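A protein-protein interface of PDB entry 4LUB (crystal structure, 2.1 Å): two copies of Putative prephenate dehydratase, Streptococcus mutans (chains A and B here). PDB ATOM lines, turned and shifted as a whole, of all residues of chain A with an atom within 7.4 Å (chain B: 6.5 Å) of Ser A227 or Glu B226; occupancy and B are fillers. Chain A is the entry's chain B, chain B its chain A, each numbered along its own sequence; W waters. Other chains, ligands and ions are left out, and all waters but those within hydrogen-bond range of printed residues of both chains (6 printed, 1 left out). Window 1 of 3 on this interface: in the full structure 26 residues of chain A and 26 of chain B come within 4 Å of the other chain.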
ATOM      1  N   SER A  60      -6.509 -15.116 -27.474  1.00  0.00           N
ATOM      2  CA  SER A  60      -6.642 -15.897 -28.702  1.00  0.00           C
ATOM      3  C   SER A  60      -7.381 -15.179 -29.820  1.00  0.00           C
ATOM      4  O   SER A  60      -8.378 -14.498 -29.589  1.00  0.00           O
ATOM      5  CB  SER A  60      -7.334 -17.222 -28.401  1.00  0.00           C
ATOM      6  OG  SER A  60      -6.403 -18.162 -27.885  1.00  0.00           O
ATOM      7  N   HIS A  62      -9.893 -15.131 -32.384  1.00  0.00           N
ATOM      8  CA  HIS A  62     -11.116 -15.881 -32.667  1.00  0.00           C
ATOM      9  C   HIS A  62     -11.177 -16.410 -34.098  1.00  0.00           C
ATOM     10  O   HIS A  62     -11.459 -17.595 -34.315  1.00  0.00           O
ATOM     11  CB  HIS A  62     -12.346 -15.018 -32.391  1.00  0.00           C
ATOM     12  CG  HIS A  62     -12.472 -14.593 -30.962  1.00  0.00           C
ATOM     13  ND1 HIS A  62     -13.368 -13.631 -30.555  1.00  0.00           N
ATOM     14  CD2 HIS A  62     -11.814 -14.995 -29.849  1.00  0.00           C
ATOM     15  CE1 HIS A  62     -13.255 -13.453 -29.250  1.00  0.00           C
ATOM     16  NE2 HIS A  62     -12.321 -14.269 -28.798  1.00  0.00           N
ATOM     17  N   ASP A  66     -11.738 -20.413 -34.899  1.00  0.00           N
ATOM     18  CA  ASP A  66     -13.027 -20.792 -35.489  1.00  0.00           C
ATOM     19  C   ASP A  66     -12.862 -21.427 -36.871  1.00  0.00           C
ATOM     20  O   ASP A  66     -13.465 -22.459 -37.161  1.00  0.00           O
ATOM     21  CB  ASP A  66     -13.994 -19.597 -35.572  1.00  0.00           C
ATOM     22  CG  ASP A  66     -14.279 -18.971 -34.210  1.00  0.00           C
ATOM     23  OD1 ASP A  66     -14.176 -19.686 -33.190  1.00  0.00           O
ATOM     24  OD2 ASP A  66     -14.637 -17.775 -34.163  1.00  0.00           O
ATOM     25  N   LEU A 208     -15.659 -31.369 -18.555  1.00  0.00           N
ATOM     26  CA  LEU A 208     -14.317 -30.850 -18.814  1.00  0.00           C
ATOM     27  C   LEU A 208     -13.260 -31.430 -17.880  1.00  0.00           C
ATOM     28  O   LEU A 208     -12.159 -31.774 -18.307  1.00  0.00           O
ATOM     29  CB  LEU A 208     -14.300 -29.327 -18.700  1.00  0.00           C
ATOM     30  CG  LEU A 208     -13.018 -28.671 -19.216  1.00  0.00           C
ATOM     31  CD1 LEU A 208     -12.697 -29.145 -20.638  1.00  0.00           C
ATOM     32  CD2 LEU A 208     -13.072 -27.139 -19.118  1.00  0.00           C
ATOM     33  N   ILE A 225      -6.076 -22.971 -22.081  1.00  0.00           N
ATOM     34  CA  ILE A 225      -7.430 -23.399 -22.382  1.00  0.00           C
ATOM     35  C   ILE A 225      -8.299 -22.207 -22.738  1.00  0.00           C
ATOM     36  O   ILE A 225      -8.320 -21.202 -22.033  1.00  0.00           O
ATOM     37  CB  ILE A 225      -8.085 -24.175 -21.232  1.00  0.00           C
ATOM     38  CG1 ILE A 225      -9.517 -24.556 -21.621  1.00  0.00           C
ATOM     39  CG2 ILE A 225      -8.068 -23.357 -19.954  1.00  0.00           C
ATOM     40  CD1 ILE A 225     -10.039 -25.790 -20.928  1.00  0.00           C
ATOM     41  N   GLU A 226      -9.008 -22.328 -23.846  1.00  0.00           N
ATOM     42  CA  GLU A 226      -9.884 -21.272 -24.301  1.00  0.00           C
ATOM     43  C   GLU A 226     -11.136 -21.899 -24.875  1.00  0.00           C
ATOM     44  O   GLU A 226     -11.060 -22.866 -25.619  1.00  0.00           O
ATOM     45  CB  GLU A 226      -9.180 -20.426 -25.358  1.00  0.00           C
ATOM     46  CG  GLU A 226      -9.998 -19.250 -25.862  1.00  0.00           C
ATOM     47  CD  GLU A 226      -9.496 -17.925 -25.335  1.00  0.00           C
ATOM     48  OE1 GLU A 226      -8.336 -17.579 -25.609  1.00  0.00           O
ATOM     49  OE2 GLU A 226     -10.261 -17.230 -24.647  1.00  0.00           O
ATOM     50  N   SER A 227     -12.287 -21.352 -24.526  1.00  0.00           N
ATOM     51  CA  SER A 227     -13.530 -21.835 -25.094  1.00  0.00           C
ATOM     52  C   SER A 227     -13.999 -20.935 -26.230  1.00  0.00           C
ATOM     53  O   SER A 227     -13.721 -19.739 -26.253  1.00  0.00           O
ATOM     54  CB  SER A 227     -14.610 -22.021 -24.024  1.00  0.00           C
ATOM     55  OG  SER A 227     -15.196 -20.798 -23.640  1.00  0.00           O
ATOM     56  N   ARG A 228     -14.697 -21.539 -27.180  1.00  0.00           N
ATOM     57  CA  ARG A 228     -15.216 -20.852 -28.345  1.00  0.00           C
ATOM     58  C   ARG A 228     -16.642 -21.339 -28.526  1.00  0.00           C
ATOM     59  O   ARG A 228     -16.931 -22.498 -28.217  1.00  0.00           O
ATOM     60  CB  ARG A 228     -14.382 -21.175 -29.590  1.00  0.00           C
ATOM     61  CG  ARG A 228     -12.943 -20.599 -29.643  1.00  0.00           C
ATOM     62  CD  ARG A 228     -12.939 -19.096 -29.466  1.00  0.00           C
ATOM     63  NE  ARG A 228     -13.683 -18.451 -30.533  1.00  0.00           N
ATOM     64  CZ  ARG A 228     -14.458 -17.387 -30.364  1.00  0.00           C
ATOM     65  NH1 ARG A 228     -14.583 -16.848 -29.157  1.00  0.00           N
ATOM     66  NH2 ARG A 228     -15.108 -16.867 -31.404  1.00  0.00           N
ATOM     67  N   PRO A 229     -17.547 -20.463 -28.987  1.00  0.00           N
ATOM     68  CA  PRO A 229     -18.907 -20.927 -29.297  1.00  0.00           C
ATOM     69  C   PRO A 229     -18.914 -22.068 -30.309  1.00  0.00           C
ATOM     70  O   PRO A 229     -18.200 -22.012 -31.312  1.00  0.00           O
ATOM     71  CB  PRO A 229     -19.594 -19.676 -29.872  1.00  0.00           C
ATOM     72  CG  PRO A 229     -18.711 -18.525 -29.486  1.00  0.00           C
ATOM     73  CD  PRO A 229     -17.326 -19.074 -29.412  1.00  0.00           C
ATOM     74  N   LEU A 230     -19.714 -23.095 -30.036  1.00  0.00           N
ATOM     75  CA  LEU A 230     -19.930 -24.183 -30.988  1.00  0.00           C
ATOM     76  C   LEU A 230     -20.757 -23.731 -32.183  1.00  0.00           C
ATOM     77  O   LEU A 230     -20.848 -24.437 -33.188  1.00  0.00           O
ATOM     78  CB  LEU A 230     -20.610 -25.368 -30.301  1.00  0.00           C
ATOM     79  CG  LEU A 230     -20.326 -26.759 -30.868  1.00  0.00           C
ATOM     80  CD1 LEU A 230     -18.851 -26.955 -31.169  1.00  0.00           C
ATOM     81  CD2 LEU A 230     -20.829 -27.833 -29.912  1.00  0.00           C
ATOM     82  N   TYR A 237     -20.015 -25.258 -26.438  1.00  0.00           N
ATOM     83  CA  TYR A 237     -18.726 -24.743 -26.841  1.00  0.00           C
ATOM     84  C   TYR A 237     -17.806 -25.846 -27.309  1.00  0.00           C
ATOM     85  O   TYR A 237     -18.037 -27.018 -27.041  1.00  0.00           O
ATOM     86  CB  TYR A 237     -18.059 -24.048 -25.655  1.00  0.00           C
ATOM     87  CG  TYR A 237     -18.933 -23.066 -24.911  1.00  0.00           C
ATOM     88  CD1 TYR A 237     -19.029 -21.749 -25.320  1.00  0.00           C
ATOM     89  CD2 TYR A 237     -19.648 -23.456 -23.787  1.00  0.00           C
ATOM     90  CE1 TYR A 237     -19.815 -20.846 -24.638  1.00  0.00           C
ATOM     91  CE2 TYR A 237     -20.438 -22.558 -23.096  1.00  0.00           C
ATOM     92  CZ  TYR A 237     -20.518 -21.252 -23.526  1.00  0.00           C
ATOM     93  OH  TYR A 237     -21.299 -20.353 -22.848  1.00  0.00           O
ATOM     94  N   PHE A 238     -16.745 -25.456 -27.993  1.00  0.00           N
ATOM     95  CA  PHE A 238     -15.599 -26.318 -28.160  1.00  0.00           C
ATOM     96  C   PHE A 238     -14.440 -25.656 -27.437  1.00  0.00           C
ATOM     97  O   PHE A 238     -14.407 -24.442 -27.280  1.00  0.00           O
ATOM     98  CB  PHE A 238     -15.297 -26.639 -29.627  1.00  0.00           C
ATOM     99  CG  PHE A 238     -14.683 -25.511 -30.404  1.00  0.00           C
ATOM    100  CD1 PHE A 238     -13.311 -25.379 -30.484  1.00  0.00           C
ATOM    101  CD2 PHE A 238     -15.477 -24.612 -31.089  1.00  0.00           C
ATOM    102  CE1 PHE A 238     -12.743 -24.358 -31.215  1.00  0.00           C
ATOM    103  CE2 PHE A 238     -14.914 -23.587 -31.823  1.00  0.00           C
ATOM    104  CZ  PHE A 238     -13.543 -23.459 -31.885  1.00  0.00           C
ATOM    105  N   PHE A 239     -13.510 -26.465 -26.967  1.00  0.00           N
ATOM    106  CA  PHE A 239     -12.406 -25.964 -26.163  1.00  0.00           C
ATOM    107  C   PHE A 239     -11.061 -26.105 -26.849  1.00  0.00           C
ATOM    108  O   PHE A 239     -10.701 -27.182 -27.309  1.00  0.00           O
ATOM    109  CB  PHE A 239     -12.400 -26.679 -24.804  1.00  0.00           C
ATOM    110  CG  PHE A 239     -13.682 -26.513 -24.046  1.00  0.00           C
ATOM    111  CD1 PHE A 239     -13.875 -25.410 -23.234  1.00  0.00           C
ATOM    112  CD2 PHE A 239     -14.711 -27.425 -24.182  1.00  0.00           C
ATOM    113  CE1 PHE A 239     -15.065 -25.236 -22.545  1.00  0.00           C
ATOM    114  CE2 PHE A 239     -15.901 -27.256 -23.496  1.00  0.00           C
ATOM    115  CZ  PHE A 239     -16.077 -26.162 -22.680  1.00  0.00           C
ATOM    116  N   ILE A 240     -10.323 -25.001 -26.904  1.00  0.00           N
ATOM    117  CA  ILE A 240      -8.938 -25.022 -27.351  1.00  0.00           C
ATOM    118  C   ILE A 240      -8.032 -25.270 -26.168  1.00  0.00           C
ATOM    119  O   ILE A 240      -7.976 -24.476 -25.236  1.00  0.00           O
ATOM    120  CB  ILE A 240      -8.515 -23.708 -28.011  1.00  0.00           C
ATOM    121  CG1 ILE A 240      -9.535 -23.307 -29.065  1.00  0.00           C
ATOM    122  CG2 ILE A 240      -7.127 -23.851 -28.627  1.00  0.00           C
ATOM    123  CD1 ILE A 240      -9.693 -24.373 -30.122  1.00  0.00           C
ATOM    124  N   ILE A 241      -7.349 -26.401 -26.207  1.00  0.00           N
ATOM    125  CA  ILE A 241      -6.391 -26.765 -25.181  1.00  0.00           C
ATOM    126  C   ILE A 241      -4.982 -27.027 -25.724  1.00  0.00           C
ATOM    127  O   ILE A 241      -4.808 -27.737 -26.713  1.00  0.00           O
ATOM    128  CB  ILE A 241      -6.932 -27.985 -24.392  1.00  0.00           C
ATOM    129  CG1 ILE A 241      -8.180 -27.580 -23.626  1.00  0.00           C
ATOM    130  CG2 ILE A 241      -5.950 -28.406 -23.323  1.00  0.00           C
ATOM    131  CD1 ILE A 241      -8.945 -28.717 -23.034  1.00  0.00           C
ATOM    132  N   GLU B  58     -18.925 -14.099 -31.193  1.00  0.00           N
ATOM    133  CA  GLU B  58     -17.626 -13.720 -30.662  1.00  0.00           C
ATOM    134  C   GLU B  58     -17.272 -14.452 -29.367  1.00  0.00           C
ATOM    135  O   GLU B  58     -16.100 -14.607 -29.050  1.00  0.00           O
ATOM    136  CB  GLU B  58     -17.574 -12.199 -30.442  1.00  0.00           C
ATOM    137  CG  GLU B  58     -17.555 -11.379 -31.725  1.00  0.00           C
ATOM    138  CD  GLU B  58     -16.247 -11.474 -32.505  1.00  0.00           C
ATOM    139  OE1 GLU B  58     -15.317 -12.175 -32.058  1.00  0.00           O
ATOM    140  OE2 GLU B  58     -16.162 -10.845 -33.582  1.00  0.00           O
ATOM    141  N   GLY B  59     -18.277 -14.878 -28.612  1.00  0.00           N
ATOM    142  CA  GLY B  59     -18.005 -15.531 -27.346  1.00  0.00           C
ATOM    143  C   GLY B  59     -18.095 -14.569 -26.176  1.00  0.00           C
ATOM    144  O   GLY B  59     -18.866 -13.605 -26.209  1.00  0.00           O
ATOM    145  N   SER B  60     -17.341 -14.860 -25.120  1.00  0.00           N
ATOM    146  CA  SER B  60     -17.302 -13.985 -23.956  1.00  0.00           C
ATOM    147  C   SER B  60     -16.746 -12.618 -24.336  1.00  0.00           C
ATOM    148  O   SER B  60     -15.775 -12.517 -25.084  1.00  0.00           O
ATOM    149  CB  SER B  60     -16.462 -14.605 -22.844  1.00  0.00           C
ATOM    150  OG  SER B  60     -17.224 -15.559 -22.113  1.00  0.00           O
ATOM    151  N   HIS B  62     -14.568  -9.714 -23.977  1.00  0.00           N
ATOM    152  CA  HIS B  62     -13.290  -9.421 -23.331  1.00  0.00           C
ATOM    153  C   HIS B  62     -13.323  -8.178 -22.444  1.00  0.00           C
ATOM    154  O   HIS B  62     -12.919  -8.231 -21.278  1.00  0.00           O
ATOM    155  CB  HIS B  62     -12.180  -9.255 -24.383  1.00  0.00           C
ATOM    156  CG  HIS B  62     -11.921 -10.486 -25.195  1.00  0.00           C
ATOM    157  ND1 HIS B  62     -11.098 -10.483 -26.302  1.00  0.00           N
ATOM    158  CD2 HIS B  62     -12.388 -11.752 -25.078  1.00  0.00           C
ATOM    159  CE1 HIS B  62     -11.060 -11.695 -26.823  1.00  0.00           C
ATOM    160  NE2 HIS B  62     -11.831 -12.486 -26.099  1.00  0.00           N
ATOM    161  N   PHE B  65     -15.219  -8.646 -18.963  1.00  0.00           N
ATOM    162  CA  PHE B  65     -14.518  -9.484 -17.999  1.00  0.00           C
ATOM    163  C   PHE B  65     -13.164  -8.921 -17.582  1.00  0.00           C
ATOM    164  O   PHE B  65     -12.813  -9.005 -16.404  1.00  0.00           O
ATOM    165  CB  PHE B  65     -14.389 -10.908 -18.543  1.00  0.00           C
ATOM    166  CG  PHE B  65     -15.689 -11.654 -18.520  1.00  0.00           C
ATOM    167  CD1 PHE B  65     -16.227 -12.087 -17.316  1.00  0.00           C
ATOM    168  CD2 PHE B  65     -16.403 -11.877 -19.685  1.00  0.00           C
ATOM    169  CE1 PHE B  65     -17.436 -12.751 -17.278  1.00  0.00           C
ATOM    170  CE2 PHE B  65     -17.624 -12.541 -19.652  1.00  0.00           C
ATOM    171  CZ  PHE B  65     -18.137 -12.978 -18.447  1.00  0.00           C
ATOM    172  N   LYS B 224     -19.820 -22.982 -17.635  1.00  0.00           N
ATOM    173  CA  LYS B 224     -18.903 -22.289 -18.535  1.00  0.00           C
ATOM    174  C   LYS B 224     -17.491 -22.248 -17.957  1.00  0.00           C
ATOM    175  O   LYS B 224     -17.306 -22.111 -16.744  1.00  0.00           O
ATOM    176  CB  LYS B 224     -19.403 -20.867 -18.831  1.00  0.00           C
ATOM    177  CG  LYS B 224     -18.541 -20.079 -19.817  1.00  0.00           C
ATOM    178  CD  LYS B 224     -18.940 -18.599 -19.881  1.00  0.00           C
ATOM    179  CE  LYS B 224     -18.071 -17.706 -19.000  1.00  0.00           C
ATOM    180  NZ  LYS B 224     -18.098 -16.293 -19.490  1.00  0.00           N
ATOM    181  N   ILE B 225     -16.502 -22.390 -18.834  1.00  0.00           N
ATOM    182  CA  ILE B 225     -15.106 -22.177 -18.472  1.00  0.00           C
ATOM    183  C   ILE B 225     -14.436 -21.375 -19.577  1.00  0.00           C
ATOM    184  O   ILE B 225     -14.370 -21.808 -20.729  1.00  0.00           O
ATOM    185  CB  ILE B 225     -14.328 -23.513 -18.257  1.00  0.00           C
ATOM    186  CG1 ILE B 225     -14.903 -24.312 -17.085  1.00  0.00           C
ATOM    187  CG2 ILE B 225     -12.848 -23.243 -17.994  1.00  0.00           C
ATOM    188  CD1 ILE B 225     -15.989 -25.298 -17.460  1.00  0.00           C
ATOM    189  N   GLU B 226     -13.948 -20.198 -19.203  1.00  0.00           N
ATOM    190  CA  GLU B 226     -13.260 -19.273 -20.102  1.00  0.00           C
ATOM    191  C   GLU B 226     -11.956 -18.789 -19.474  1.00  0.00           C
ATOM    192  O   GLU B 226     -11.822 -18.758 -18.248  1.00  0.00           O
ATOM    193  CB  GLU B 226     -14.161 -18.083 -20.448  1.00  0.00           C
ATOM    194  CG  GLU B 226     -13.601 -17.115 -21.500  1.00  0.00           C
ATOM    195  CD  GLU B 226     -13.318 -17.748 -22.861  1.00  0.00           C
ATOM    196  OE1 GLU B 226     -13.993 -17.349 -23.832  1.00  0.00           O
ATOM    197  OE2 GLU B 226     -12.407 -18.607 -22.972  1.00  0.00           O
ATOM    198  N   SER B 227     -10.969 -18.474 -20.298  1.00  0.00           N
ATOM    199  CA  SER B 227      -9.795 -17.795 -19.779  1.00  0.00           C
ATOM    200  C   SER B 227      -9.550 -16.459 -20.467  1.00  0.00           C
ATOM    201  O   SER B 227     -10.039 -16.202 -21.567  1.00  0.00           O
ATOM    202  CB  SER B 227      -8.562 -18.689 -19.901  1.00  0.00           C
ATOM    203  OG  SER B 227      -8.000 -18.627 -21.185  1.00  0.00           O
ATOM    204  N   ARG B 228      -8.779 -15.620 -19.790  1.00  0.00           N
ATOM    205  CA  ARG B 228      -8.380 -14.300 -20.269  1.00  0.00           C
ATOM    206  C   ARG B 228      -6.929 -14.137 -19.853  1.00  0.00           C
ATOM    207  O   ARG B 228      -6.538 -14.623 -18.785  1.00  0.00           O
ATOM    208  CB  ARG B 228      -9.240 -13.188 -19.662  1.00  0.00           C
ATOM    209  CG  ARG B 228     -10.680 -13.062 -20.193  1.00  0.00           C
ATOM    210  CD  ARG B 228     -10.708 -12.797 -21.704  1.00  0.00           C
ATOM    211  NE  ARG B 228     -10.058 -11.525 -21.994  1.00  0.00           N
ATOM    212  CZ  ARG B 228      -9.324 -11.265 -23.071  1.00  0.00           C
ATOM    213  NH1 ARG B 228      -9.156 -12.186 -24.010  1.00  0.00           N
ATOM    214  NH2 ARG B 228      -8.776 -10.063 -23.215  1.00  0.00           N
ATOM    215  N   PHE B 238      -6.140 -15.657 -16.086  1.00  0.00           N
ATOM    216  CA  PHE B 238      -7.133 -15.890 -15.053  1.00  0.00           C
ATOM    217  C   PHE B 238      -8.296 -16.651 -15.685  1.00  0.00           C
ATOM    218  O   PHE B 238      -8.537 -16.535 -16.878  1.00  0.00           O
ATOM    219  CB  PHE B 238      -7.569 -14.600 -14.346  1.00  0.00           C
ATOM    220  CG  PHE B 238      -8.457 -13.703 -15.163  1.00  0.00           C
ATOM    221  CD1 PHE B 238      -9.833 -13.863 -15.152  1.00  0.00           C
ATOM    222  CD2 PHE B 238      -7.917 -12.667 -15.902  1.00  0.00           C
ATOM    223  CE1 PHE B 238     -10.648 -13.020 -15.887  1.00  0.00           C
ATOM    224  CE2 PHE B 238      -8.726 -11.822 -16.637  1.00  0.00           C
ATOM    225  CZ  PHE B 238     -10.093 -11.997 -16.631  1.00  0.00           C
ATOM    226  N   PHE B 239      -8.982 -17.463 -14.889  1.00  0.00           N
ATOM    227  CA  PHE B 239     -10.028 -18.342 -15.408  1.00  0.00           C
ATOM    228  C   PHE B 239     -11.413 -17.999 -14.860  1.00  0.00           C
ATOM    229  O   PHE B 239     -11.610 -17.921 -13.649  1.00  0.00           O
ATOM    230  CB  PHE B 239      -9.652 -19.791 -15.083  1.00  0.00           C
ATOM    231  CG  PHE B 239      -8.282 -20.168 -15.591  1.00  0.00           C
ATOM    232  CD1 PHE B 239      -8.108 -20.622 -16.885  1.00  0.00           C
ATOM    233  CD2 PHE B 239      -7.161 -19.976 -14.797  1.00  0.00           C
ATOM    234  CE1 PHE B 239      -6.843 -20.928 -17.360  1.00  0.00           C
ATOM    235  CE2 PHE B 239      -5.900 -20.284 -15.265  1.00  0.00           C
ATOM    236  CZ  PHE B 239      -5.744 -20.759 -16.551  1.00  0.00           C
ATOM    237  N   ILE B 240     -12.365 -17.785 -15.761  1.00  0.00           N
ATOM    238  CA  ILE B 240     -13.770 -17.586 -15.393  1.00  0.00           C
ATOM    239  C   ILE B 240     -14.609 -18.852 -15.429  1.00  0.00           C
ATOM    240  O   ILE B 240     -14.750 -19.471 -16.476  1.00  0.00           O
ATOM    241  CB  ILE B 240     -14.444 -16.556 -16.319  1.00  0.00           C
ATOM    242  CG1 ILE B 240     -13.563 -15.308 -16.452  1.00  0.00           C
ATOM    243  CG2 ILE B 240     -15.841 -16.202 -15.798  1.00  0.00           C
ATOM    244  CD1 ILE B 240     -13.633 -14.668 -17.825  1.00  0.00           C
ATOM    245  N   ILE B 241     -15.152 -19.246 -14.282  1.00  0.00           N
ATOM    246  CA  ILE B 241     -16.060 -20.381 -14.245  1.00  0.00           C
ATOM    247  C   ILE B 241     -17.436 -19.971 -13.711  1.00  0.00           C
ATOM    248  O   ILE B 241     -17.546 -19.229 -12.730  1.00  0.00           O
ATOM    249  CB  ILE B 241     -15.460 -21.567 -13.411  1.00  0.00           C
ATOM    250  CG1 ILE B 241     -15.437 -21.234 -11.916  1.00  0.00           C
ATOM    251  CG2 ILE B 241     -14.039 -21.876 -13.865  1.00  0.00           C
ATOM    252  CD1 ILE B 241     -15.288 -22.453 -11.018  1.00  0.00           C
HETATM  253  O   HOH W   1      -8.758 -15.035 -24.417  1.00  0.00           O
HETATM  254  O   HOH W   2      -5.585 -20.401 -20.811  1.00  0.00           O
HETATM  255  O   HOH W   3     -17.294 -22.548 -21.653  1.00  0.00           O
HETATM  256  O   HOH W   4      -7.073 -16.189 -22.689  1.00  0.00           O
HETATM  257  O   HOH W   5     -13.609 -14.366 -26.395  1.00  0.00           O
HETATM  258  O   HOH W   6      -9.634 -14.880 -27.061  1.00  0.00           O
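OE1 of Glu B58 sits at hydrogen-bond distance from ND1 of His A62 (2.9 Å).
O of Glu B58 sits at hydrogen-bond distance from NH1 of Arg A228, 2.7 Å away.
NE2 of His B62 is in hydrogen-bond range of NE2 of His A62 (3.3 Å).
The backbone carbonyl oxygen of Ile B225 is in hydrogen-bond range of the side-chain hydroxyl of Ser A227.
OE2 of Glu B226 lies within hydrogen-bond range of N of Ser A227, 3.2 Å away.
The side-chain hydroxyl (OG) of Ser B227 is in hydrogen-bond range of the backbone carbonyl oxygen (O) of Ile A225, at 2.7 Å.
The side-chain carboxylate of Glu A226 lies close to the side-chain carboxylate of Glu B226 (3.1 Å).
The side-chain carboxylate (OE2) of Glu A226 sits close to the backbone carbonyl oxygen (O) of Ser B227 (3.3 Å).
The backbone carbonyl oxygen of Glu B226 lies within hydrogen-bond range of the backbone NH of Ile B240 (2.7 Å).
OG of Ser A60 sits close to OE1 of Glu A226.
A ring nitrogen (NE2) of His A62 sits close to the guanidinium group (NH1) of Arg A228.
The guanidinium group of Arg A228 lies within salt-bridge range of the side-chain carboxylate of Asp A66 (2.9 Å).
The backbone carbonyl oxygen of Glu A226 lies within hydrogen-bond range of the backbone NH of Ile A240 (2.6 Å).
The backbone carbonyl oxygen (O) of Phe A238 is in hydrogen-bond range of the backbone NH (N) of Arg A228 (2.9 Å).
Among the printed residues, merely in contact across the chains: Pro A229 with Gly B59, Ile A225 with Phe B239, Leu A208 with Ile B225 and Phe A239 with Ile B225.
Glu B226 touches two residues of chain A.
Printed residues of chain B within 4 Å of Pro A229: Gly B59.
Printed residues of chain A within 4 Å of Glu B58: His A62 (2.9 Å) and Arg A228 (2.7 Å).
Ile A241 touches none of the printed residues of chain B.
The nearest residue of chain B that does not touch Ser A227 is Lys B224 (5.1 Å).
The nearest printed residue of chain A that does not touch His B62 is Ser A60 (4.8 Å).
Hydrophobic or aromatic side chains of chain B that line the printed part of chain A: His B62, Ile B225 and Phe B239.
Along chain B the printed residues that touch a printed residue of chain A span positions 58 to 239.
Printed residues of chain A that touch a printed residue of chain B: His A62, Leu A208, Ile A225, Glu A226, Ser A227, Arg A228, Pro A229 and Phe A239.
Among the printed residues, 12 pairs touch across the chains.
Among the printed residues, no Asp or Glu carboxylate lies within 4 Å of a Lys or Arg side-chain nitrogen of the other chain.
His B62 touches its own counterpart, His A62.
Ile A225 touches Ser B227, and with the chains exchanged Ser A227 touches Ile B225.
Ile A225 touches Phe B239, and with the chains exchanged Phe A239 touches Ile B225.
Glu B226 touches its own counterpart, Glu A226.
Positions printed for both chains: 60, 62, 225, 226, 227, 228, 238, 239, 240 and 241.
Of the 12 pairs that touch across the chains among the printed residues, 8 have their exchanged pair printed and touching as well.
Water W5 lies within hydrogen-bond range of NE2 of His B62 (2.6 Å), NE2 of His A62 (2.7 Å) and O of Ser B60 (3.1 Å).
Water W1 lies within hydrogen-bond range of the side-chain carboxylate (OE2) of Glu A226 (2.7 Å), the guanidinium group (NH1) of Arg B228 (2.9 Å) and the backbone carbonyl oxygen (O) of Ser B227 (3.3 Å).
Water W6 lies within hydrogen-bond range of the backbone carbonyl oxygen of Ser A60 (2.8 Å), a ring nitrogen (NE2) of His A62 (3.3 Å), the side-chain carboxylate of Glu A226 (3.3 Å) and a ring nitrogen (NE2) of His B62 (3.4 Å).
Water W2 bridges N of Ile A225 and OG of Ser B227.
Water W3 bridges the backbone NH of Ile B225 (2.9 Å) and the side-chain hydroxyl of Ser A227 (3.4 Å).
Water W4 lies within hydrogen-bond range of the side-chain hydroxyl (OG) of Ser B227 (3.0 Å), the backbone NH (N) of Arg B228 (3.4 Å) and the side-chain carboxylate (OE1) of Glu A226 (3.5 Å).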
